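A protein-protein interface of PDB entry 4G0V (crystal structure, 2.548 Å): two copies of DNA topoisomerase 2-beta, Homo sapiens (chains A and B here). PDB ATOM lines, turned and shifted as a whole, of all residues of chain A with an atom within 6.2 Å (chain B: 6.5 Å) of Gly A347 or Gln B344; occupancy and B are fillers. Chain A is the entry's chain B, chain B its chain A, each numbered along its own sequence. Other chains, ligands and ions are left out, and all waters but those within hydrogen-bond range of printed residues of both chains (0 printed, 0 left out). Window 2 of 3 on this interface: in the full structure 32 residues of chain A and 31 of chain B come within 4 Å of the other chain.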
ATOM      1  N   ARG A 334      26.000 -39.178 -13.169  1.00  0.00           N
ATOM      2  CA  ARG A 334      24.888 -39.087 -12.236  1.00  0.00           C
ATOM      3  C   ARG A 334      23.983 -40.298 -12.279  1.00  0.00           C
ATOM      4  O   ARG A 334      23.548 -40.793 -11.249  1.00  0.00           O
ATOM      5  CB  ARG A 334      24.015 -37.901 -12.594  1.00  0.00           C
ATOM      6  CG  ARG A 334      24.477 -36.558 -12.114  1.00  0.00           C
ATOM      7  CD  ARG A 334      23.317 -35.573 -12.285  1.00  0.00           C
ATOM      8  NE  ARG A 334      23.269 -34.605 -11.195  1.00  0.00           N
ATOM      9  CZ  ARG A 334      22.350 -34.577 -10.237  1.00  0.00           C
ATOM     10  NH1 ARG A 334      21.361 -35.463 -10.211  1.00  0.00           N
ATOM     11  NH2 ARG A 334      22.418 -33.637  -9.308  1.00  0.00           N
ATOM     12  N   VAL A 342      16.143 -28.829 -13.966  1.00  0.00           N
ATOM     13  CA  VAL A 342      17.133 -28.365 -14.939  1.00  0.00           C
ATOM     14  C   VAL A 342      18.191 -27.453 -14.310  1.00  0.00           C
ATOM     15  O   VAL A 342      19.397 -27.665 -14.503  1.00  0.00           O
ATOM     16  CB  VAL A 342      16.451 -27.710 -16.168  1.00  0.00           C
ATOM     17  CG1 VAL A 342      17.448 -26.945 -17.022  1.00  0.00           C
ATOM     18  CG2 VAL A 342      15.726 -28.768 -16.993  1.00  0.00           C
ATOM     19  N   ALA A 343      17.758 -26.470 -13.525  1.00  0.00           N
ATOM     20  CA  ALA A 343      18.712 -25.612 -12.827  1.00  0.00           C
ATOM     21  C   ALA A 343      19.642 -26.404 -11.885  1.00  0.00           C
ATOM     22  O   ALA A 343      20.837 -26.109 -11.761  1.00  0.00           O
ATOM     23  CB  ALA A 343      17.993 -24.509 -12.086  1.00  0.00           C
ATOM     24  N   GLN A 344      19.115 -27.425 -11.228  1.00  0.00           N
ATOM     25  CA  GLN A 344      19.983 -28.231 -10.396  1.00  0.00           C
ATOM     26  C   GLN A 344      20.970 -29.002 -11.266  1.00  0.00           C
ATOM     27  O   GLN A 344      22.164 -29.048 -10.950  1.00  0.00           O
ATOM     28  CB  GLN A 344      19.177 -29.154  -9.472  1.00  0.00           C
ATOM     29  CG  GLN A 344      20.016 -29.913  -8.415  1.00  0.00           C
ATOM     30  CD  GLN A 344      20.730 -29.014  -7.368  1.00  0.00           C
ATOM     31  OE1 GLN A 344      20.752 -27.769  -7.469  1.00  0.00           O
ATOM     32  NE2 GLN A 344      21.322 -29.662  -6.358  1.00  0.00           N
ATOM     33  N   LEU A 345      20.489 -29.584 -12.372  1.00  0.00           N
ATOM     34  CA  LEU A 345      21.382 -30.302 -13.286  1.00  0.00           C
ATOM     35  C   LEU A 345      22.531 -29.404 -13.770  1.00  0.00           C
ATOM     36  O   LEU A 345      23.695 -29.814 -13.766  1.00  0.00           O
ATOM     37  CB  LEU A 345      20.620 -30.892 -14.477  1.00  0.00           C
ATOM     38  CG  LEU A 345      21.457 -31.726 -15.464  1.00  0.00           C
ATOM     39  CD1 LEU A 345      22.144 -32.888 -14.761  1.00  0.00           C
ATOM     40  CD2 LEU A 345      20.614 -32.241 -16.631  1.00  0.00           C
ATOM     41  N   ALA A 346      22.207 -28.177 -14.160  1.00  0.00           N
ATOM     42  CA  ALA A 346      23.225 -27.248 -14.621  1.00  0.00           C
ATOM     43  C   ALA A 346      24.327 -27.036 -13.587  1.00  0.00           C
ATOM     44  O   ALA A 346      25.522 -27.109 -13.918  1.00  0.00           O
ATOM     45  CB  ALA A 346      22.600 -25.942 -14.991  1.00  0.00           C
ATOM     46  N   GLY A 347      23.922 -26.773 -12.341  1.00  0.00           N
ATOM     47  CA  GLY A 347      24.863 -26.618 -11.247  1.00  0.00           C
ATOM     48  C   GLY A 347      25.732 -27.845 -11.068  1.00  0.00           C
ATOM     49  O   GLY A 347      26.925 -27.741 -10.802  1.00  0.00           O
ATOM     50  N   SER A 348      25.125 -29.013 -11.231  1.00  0.00           N
ATOM     51  CA  SER A 348      25.824 -30.293 -11.154  1.00  0.00           C
ATOM     52  C   SER A 348      26.844 -30.453 -12.289  1.00  0.00           C
ATOM     53  O   SER A 348      27.977 -30.876 -12.052  1.00  0.00           O
ATOM     54  CB  SER A 348      24.794 -31.423 -11.208  1.00  0.00           C
ATOM     55  OG  SER A 348      25.328 -32.656 -10.794  1.00  0.00           O
ATOM     56  N   VAL A 349      26.437 -30.119 -13.519  1.00  0.00           N
ATOM     57  CA  VAL A 349      27.359 -30.113 -14.650  1.00  0.00           C
ATOM     58  C   VAL A 349      28.528 -29.163 -14.374  1.00  0.00           C
ATOM     59  O   VAL A 349      29.689 -29.505 -14.604  1.00  0.00           O
ATOM     60  CB  VAL A 349      26.658 -29.708 -15.991  1.00  0.00           C
ATOM     61  CG1 VAL A 349      27.677 -29.575 -17.126  1.00  0.00           C
ATOM     62  CG2 VAL A 349      25.568 -30.708 -16.364  1.00  0.00           C
ATOM     63  N   ALA A 350      28.218 -27.969 -13.879  1.00  0.00           N
ATOM     64  CA  ALA A 350      29.256 -26.975 -13.592  1.00  0.00           C
ATOM     65  C   ALA A 350      30.304 -27.564 -12.677  1.00  0.00           C
ATOM     66  O   ALA A 350      31.493 -27.477 -12.960  1.00  0.00           O
ATOM     67  CB  ALA A 350      28.659 -25.737 -12.969  1.00  0.00           C
ATOM     68  N   GLU A 351      29.836 -28.190 -11.599  1.00  0.00           N
ATOM     69  CA  GLU A 351      30.669 -28.848 -10.586  1.00  0.00           C
ATOM     70  C   GLU A 351      31.470 -30.022 -11.173  1.00  0.00           C
ATOM     71  O   GLU A 351      32.703 -30.019 -11.150  1.00  0.00           O
ATOM     72  CB  GLU A 351      29.745 -29.356  -9.463  1.00  0.00           C
ATOM     73  CG  GLU A 351      30.250 -29.280  -8.028  1.00  0.00           C
ATOM     74  CD  GLU A 351      29.095 -29.396  -7.005  1.00  0.00           C
ATOM     75  OE1 GLU A 351      29.330 -29.910  -5.880  1.00  0.00           O
ATOM     76  OE2 GLU A 351      27.951 -28.963  -7.322  1.00  0.00           O
ATOM     77  N   MET A 352      30.771 -31.012 -11.729  1.00  0.00           N
ATOM     78  CA  MET A 352      31.415 -32.238 -12.207  1.00  0.00           C
ATOM     79  C   MET A 352      32.243 -32.136 -13.484  1.00  0.00           C
ATOM     80  O   MET A 352      33.092 -32.990 -13.735  1.00  0.00           O
ATOM     81  CB  MET A 352      30.396 -33.340 -12.396  1.00  0.00           C
ATOM     82  CG  MET A 352      29.809 -33.850 -11.123  1.00  0.00           C
ATOM     83  SD  MET A 352      28.746 -35.264 -11.469  1.00  0.00           S
ATOM     84  CE  MET A 352      27.443 -34.947 -10.291  1.00  0.00           C
ATOM     85  N   GLU A 359      25.777 -20.025 -15.680  1.00  0.00           N
ATOM     86  CA  GLU A 359      24.928 -21.198 -15.690  1.00  0.00           C
ATOM     87  C   GLU A 359      23.687 -21.049 -16.553  1.00  0.00           C
ATOM     88  O   GLU A 359      23.123 -22.049 -16.977  1.00  0.00           O
ATOM     89  CB  GLU A 359      24.558 -21.614 -14.263  1.00  0.00           C
ATOM     90  CG  GLU A 359      25.634 -22.455 -13.582  1.00  0.00           C
ATOM     91  CD  GLU A 359      25.238 -22.895 -12.178  1.00  0.00           C
ATOM     92  OE1 GLU A 359      24.014 -22.991 -11.909  1.00  0.00           O
ATOM     93  OE2 GLU A 359      26.151 -23.130 -11.348  1.00  0.00           O
ATOM     94  N   LEU A 362      24.045 -22.740 -19.762  1.00  0.00           N
ATOM     95  CA  LEU A 362      24.017 -24.182 -19.626  1.00  0.00           C
ATOM     96  C   LEU A 362      22.587 -24.704 -19.457  1.00  0.00           C
ATOM     97  O   LEU A 362      22.235 -25.754 -19.992  1.00  0.00           O
ATOM     98  CB  LEU A 362      24.866 -24.578 -18.439  1.00  0.00           C
ATOM     99  CG  LEU A 362      25.381 -26.000 -18.424  1.00  0.00           C
ATOM    100  CD1 LEU A 362      26.084 -26.302 -19.724  1.00  0.00           C
ATOM    101  CD2 LEU A 362      26.339 -26.146 -17.260  1.00  0.00           C
ATOM    102  N   MET A 363      21.757 -23.971 -18.726  1.00  0.00           N
ATOM    103  CA  MET A 363      20.365 -24.364 -18.569  1.00  0.00           C
ATOM    104  C   MET A 363      19.640 -24.290 -19.912  1.00  0.00           C
ATOM    105  O   MET A 363      18.756 -25.105 -20.204  1.00  0.00           O
ATOM    106  CB  MET A 363      19.656 -23.490 -17.532  1.00  0.00           C
ATOM    107  CG  MET A 363      20.212 -23.619 -16.117  1.00  0.00           C
ATOM    108  SD  MET A 363      19.544 -22.398 -14.947  1.00  0.00           S
ATOM    109  CE  MET A 363      20.918 -22.255 -13.821  1.00  0.00           C
ATOM    110  N   ARG B 334      24.557 -33.961   3.565  1.00  0.00           N
ATOM    111  CA  ARG B 334      25.565 -33.929   2.523  1.00  0.00           C
ATOM    112  C   ARG B 334      26.946 -34.182   3.090  1.00  0.00           C
ATOM    113  O   ARG B 334      27.737 -34.907   2.505  1.00  0.00           O
ATOM    114  CB  ARG B 334      25.600 -32.564   1.855  1.00  0.00           C
ATOM    115  CG  ARG B 334      24.402 -32.202   1.046  1.00  0.00           C
ATOM    116  CD  ARG B 334      24.613 -30.803   0.511  1.00  0.00           C
ATOM    117  NE  ARG B 334      24.322 -30.744  -0.906  1.00  0.00           N
ATOM    118  CZ  ARG B 334      25.234 -30.677  -1.863  1.00  0.00           C
ATOM    119  NH1 ARG B 334      26.529 -30.645  -1.571  1.00  0.00           N
ATOM    120  NH2 ARG B 334      24.833 -30.627  -3.120  1.00  0.00           N
ATOM    121  N   VAL B 340      30.379 -25.345  -1.458  1.00  0.00           N
ATOM    122  CA  VAL B 340      29.308 -25.539  -2.418  1.00  0.00           C
ATOM    123  C   VAL B 340      28.720 -24.181  -2.815  1.00  0.00           C
ATOM    124  O   VAL B 340      28.516 -23.327  -1.947  1.00  0.00           O
ATOM    125  CB  VAL B 340      28.169 -26.335  -1.789  1.00  0.00           C
ATOM    126  CG1 VAL B 340      27.092 -26.574  -2.807  1.00  0.00           C
ATOM    127  CG2 VAL B 340      28.680 -27.641  -1.260  1.00  0.00           C
ATOM    128  N   LYS B 341      28.440 -23.972  -4.102  1.00  0.00           N
ATOM    129  CA  LYS B 341      27.725 -22.768  -4.543  1.00  0.00           C
ATOM    130  C   LYS B 341      26.426 -22.628  -3.759  1.00  0.00           C
ATOM    131  O   LYS B 341      25.676 -23.597  -3.589  1.00  0.00           O
ATOM    132  CB  LYS B 341      27.393 -22.826  -6.035  1.00  0.00           C
ATOM    133  CG  LYS B 341      28.286 -22.009  -6.952  1.00  0.00           C
ATOM    134  CD  LYS B 341      27.836 -22.205  -8.409  1.00  0.00           C
ATOM    135  CE  LYS B 341      28.976 -22.055  -9.421  1.00  0.00           C
ATOM    136  NZ  LYS B 341      28.546 -22.364 -10.844  1.00  0.00           N
ATOM    137  N   VAL B 342      26.156 -21.424  -3.277  1.00  0.00           N
ATOM    138  CA  VAL B 342      24.940 -21.203  -2.511  1.00  0.00           C
ATOM    139  C   VAL B 342      23.710 -21.621  -3.303  1.00  0.00           C
ATOM    140  O   VAL B 342      22.829 -22.309  -2.776  1.00  0.00           O
ATOM    141  CB  VAL B 342      24.840 -19.752  -2.029  1.00  0.00           C
ATOM    142  CG1 VAL B 342      23.401 -19.411  -1.613  1.00  0.00           C
ATOM    143  CG2 VAL B 342      25.844 -19.531  -0.897  1.00  0.00           C
ATOM    144  N   ALA B 343      23.685 -21.254  -4.584  1.00  0.00           N
ATOM    145  CA  ALA B 343      22.583 -21.611  -5.481  1.00  0.00           C
ATOM    146  C   ALA B 343      22.436 -23.130  -5.614  1.00  0.00           C
ATOM    147  O   ALA B 343      21.324 -23.666  -5.590  1.00  0.00           O
ATOM    148  CB  ALA B 343      22.768 -20.960  -6.837  1.00  0.00           C
ATOM    149  N   GLN B 344      23.556 -23.832  -5.727  1.00  0.00           N
ATOM    150  CA  GLN B 344      23.490 -25.279  -5.822  1.00  0.00           C
ATOM    151  C   GLN B 344      23.010 -25.895  -4.520  1.00  0.00           C
ATOM    152  O   GLN B 344      22.188 -26.822  -4.535  1.00  0.00           O
ATOM    153  CB  GLN B 344      24.831 -25.885  -6.259  1.00  0.00           C
ATOM    154  CG  GLN B 344      24.796 -27.393  -6.545  1.00  0.00           C
ATOM    155  CD  GLN B 344      23.884 -27.781  -7.716  1.00  0.00           C
ATOM    156  OE1 GLN B 344      23.688 -28.963  -7.981  1.00  0.00           O
ATOM    157  NE2 GLN B 344      23.342 -26.793  -8.422  1.00  0.00           N
ATOM    158  N   LEU B 345      23.499 -25.375  -3.391  1.00  0.00           N
ATOM    159  CA  LEU B 345      23.047 -25.861  -2.094  1.00  0.00           C
ATOM    160  C   LEU B 345      21.537 -25.672  -1.959  1.00  0.00           C
ATOM    161  O   LEU B 345      20.826 -26.568  -1.507  1.00  0.00           O
ATOM    162  CB  LEU B 345      23.772 -25.146  -0.968  1.00  0.00           C
ATOM    163  CG  LEU B 345      23.327 -25.528   0.444  1.00  0.00           C
ATOM    164  CD1 LEU B 345      23.587 -26.998   0.751  1.00  0.00           C
ATOM    165  CD2 LEU B 345      24.027 -24.628   1.472  1.00  0.00           C
ATOM    166  N   ALA B 346      21.045 -24.512  -2.384  1.00  0.00           N
ATOM    167  CA  ALA B 346      19.612 -24.250  -2.329  1.00  0.00           C
ATOM    168  C   ALA B 346      18.788 -25.290  -3.106  1.00  0.00           C
ATOM    169  O   ALA B 346      17.767 -25.769  -2.603  1.00  0.00           O
ATOM    170  CB  ALA B 346      19.319 -22.869  -2.808  1.00  0.00           C
ATOM    171  N   GLY B 347      19.227 -25.640  -4.322  1.00  0.00           N
ATOM    172  CA  GLY B 347      18.565 -26.670  -5.097  1.00  0.00           C
ATOM    173  C   GLY B 347      18.563 -28.015  -4.386  1.00  0.00           C
ATOM    174  O   GLY B 347      17.569 -28.753  -4.398  1.00  0.00           O
ATOM    175  N   SER B 348      19.687 -28.322  -3.750  1.00  0.00           N
ATOM    176  CA  SER B 348      19.853 -29.532  -2.953  1.00  0.00           C
ATOM    177  C   SER B 348      18.931 -29.583  -1.723  1.00  0.00           C
ATOM    178  O   SER B 348      18.414 -30.643  -1.383  1.00  0.00           O
ATOM    179  CB  SER B 348      21.306 -29.638  -2.520  1.00  0.00           C
ATOM    180  OG  SER B 348      21.696 -30.982  -2.421  1.00  0.00           O
ATOM    181  N   VAL B 349      18.734 -28.449  -1.052  1.00  0.00           N
ATOM    182  CA  VAL B 349      17.778 -28.385   0.047  1.00  0.00           C
ATOM    183  C   VAL B 349      16.368 -28.651  -0.465  1.00  0.00           C
ATOM    184  O   VAL B 349      15.626 -29.444   0.108  1.00  0.00           O
ATOM    185  CB  VAL B 349      17.790 -27.001   0.764  1.00  0.00           C
ATOM    186  CG1 VAL B 349      16.696 -26.936   1.833  1.00  0.00           C
ATOM    187  CG2 VAL B 349      19.157 -26.707   1.365  1.00  0.00           C
ATOM    188  N   MET B 363      17.975 -19.189  -0.987  1.00  0.00           N
ATOM    189  CA  MET B 363      19.315 -18.643  -1.163  1.00  0.00           C
ATOM    190  C   MET B 363      19.549 -17.478  -0.213  1.00  0.00           C
ATOM    191  O   MET B 363      20.616 -17.361   0.381  1.00  0.00           O
ATOM    192  CB  MET B 363      19.556 -18.229  -2.608  1.00  0.00           C
ATOM    193  CG  MET B 363      19.615 -19.416  -3.579  1.00  0.00           C
ATOM    194  SD  MET B 363      19.502 -18.900  -5.306  1.00  0.00           S
ATOM    195  CE  MET B 363      18.948 -20.445  -6.031  1.00  0.00           C
ATOM    196  N   PRO B 401      24.024 -15.386  -5.168  1.00  0.00           N
ATOM    197  CA  PRO B 401      24.149 -16.752  -4.640  1.00  0.00           C
ATOM    198  C   PRO B 401      24.793 -17.690  -5.648  1.00  0.00           C
ATOM    199  O   PRO B 401      25.124 -18.829  -5.341  1.00  0.00           O
ATOM    200  CB  PRO B 401      22.698 -17.164  -4.401  1.00  0.00           C
ATOM    201  CG  PRO B 401      21.906 -16.281  -5.299  1.00  0.00           C
ATOM    202  CD  PRO B 401      22.618 -14.971  -5.242  1.00  0.00           C
ATOM    203  N   ARG B 402      24.998 -17.186  -6.848  1.00  0.00           N
ATOM    204  CA  ARG B 402      25.504 -18.003  -7.936  1.00  0.00           C
ATOM    205  C   ARG B 402      27.036 -17.876  -8.028  1.00  0.00           C
ATOM    206  O   ARG B 402      27.693 -18.599  -8.782  1.00  0.00           O
ATOM    207  CB  ARG B 402      24.783 -17.561  -9.213  1.00  0.00           C
ATOM    208  CG  ARG B 402      25.085 -18.336 -10.442  1.00  0.00           C
ATOM    209  CD  ARG B 402      24.971 -19.829 -10.254  1.00  0.00           C
ATOM    210  NE  ARG B 402      23.596 -20.342 -10.184  1.00  0.00           N
ATOM    211  CZ  ARG B 402      22.661 -20.228 -11.134  1.00  0.00           C
ATOM    212  NH1 ARG B 402      22.898 -19.563 -12.265  1.00  0.00           N
ATOM    213  NH2 ARG B 402      21.465 -20.772 -10.930  1.00  0.00           N
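Gln B344 touches its own counterpart, Gln A344. Gln A344 touches Gly B347, and with the chains exchanged Gly A347 touches Gln B344. Gln A344 touches Ser B348, and with the chains exchanged Ser A348 touches Gln B344. Positions printed for both chains: 334, 342, 343, 344, 345, 346, 347, 348, 349 and 363. Of the 10 pairs that touch across the chains among the printed residues, 5 have their exchanged pair printed and touching as well.
Of the printed residues of chain B, Gly A347 touches Gln B344. Printed residues of chain B within 4 Å of Glu A359: Lys B341 and Arg B402. Of the printed residues of chain B, Glu A351 touches Gln B344 (3.6 Å). Printed residues of chain B within 4 Å of Ser A348: Gln B344. Of the printed residues of chain B, Met A363 touches Arg B402 (3.3 Å). Printed residues of chain A within 4 Å of Arg B402: Glu A359 (3.2 Å) and Met A363 (3.3 Å). The nearest printed residue of chain B that does not touch Gly A347 is Lys B341 (5.6 Å). The nearest printed residue of chain A that does not touch Gln B344 is Ala A343 (4.2 Å).
The guanidinium group (NE) of Arg B334 lies within hydrogen-bond range of the side-chain hydroxyl (OG) of Ser B348 (3.0 Å). The guanidinium group (NE) of Arg A334 is in hydrogen-bond range of the side-chain hydroxyl (OG) of Ser A348 (2.9 Å).
Of the 15 printed residues of chain A, 7 touch a printed residue of chain B. Printed residues of chain B that touch a printed residue of chain A: Lys B341, Gln B344, Gly B347, Ser B348 and Arg B402.
The side-chain amino group (NZ) of Lys B341 is in salt-bridge range of the side-chain carboxylate (OE2) of Glu A359. NE2 of Gln B344 is in hydrogen-bond range of OE1 of Gln A344 (2.9 Å). N of Ser B348 lies close to NE2 of Gln A344. The guanidinium group (NE) of Arg B402 lies within salt-bridge range of the side-chain carboxylate (OE1) of Glu A359.
Gln A344 touches Gly B347 (OE1 to CA, 3.4 Å). Gly A347 touches Gln B344 (CA to NE2, 3.2 Å). Ser A348 touches Gln B344. CB of Ala A350 touches NZ of Lys B341, at 3.99 Å. Gln B344 touches Glu A351. CE of Met A363 touches NH2 of Arg B402, at 3.3 Å.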
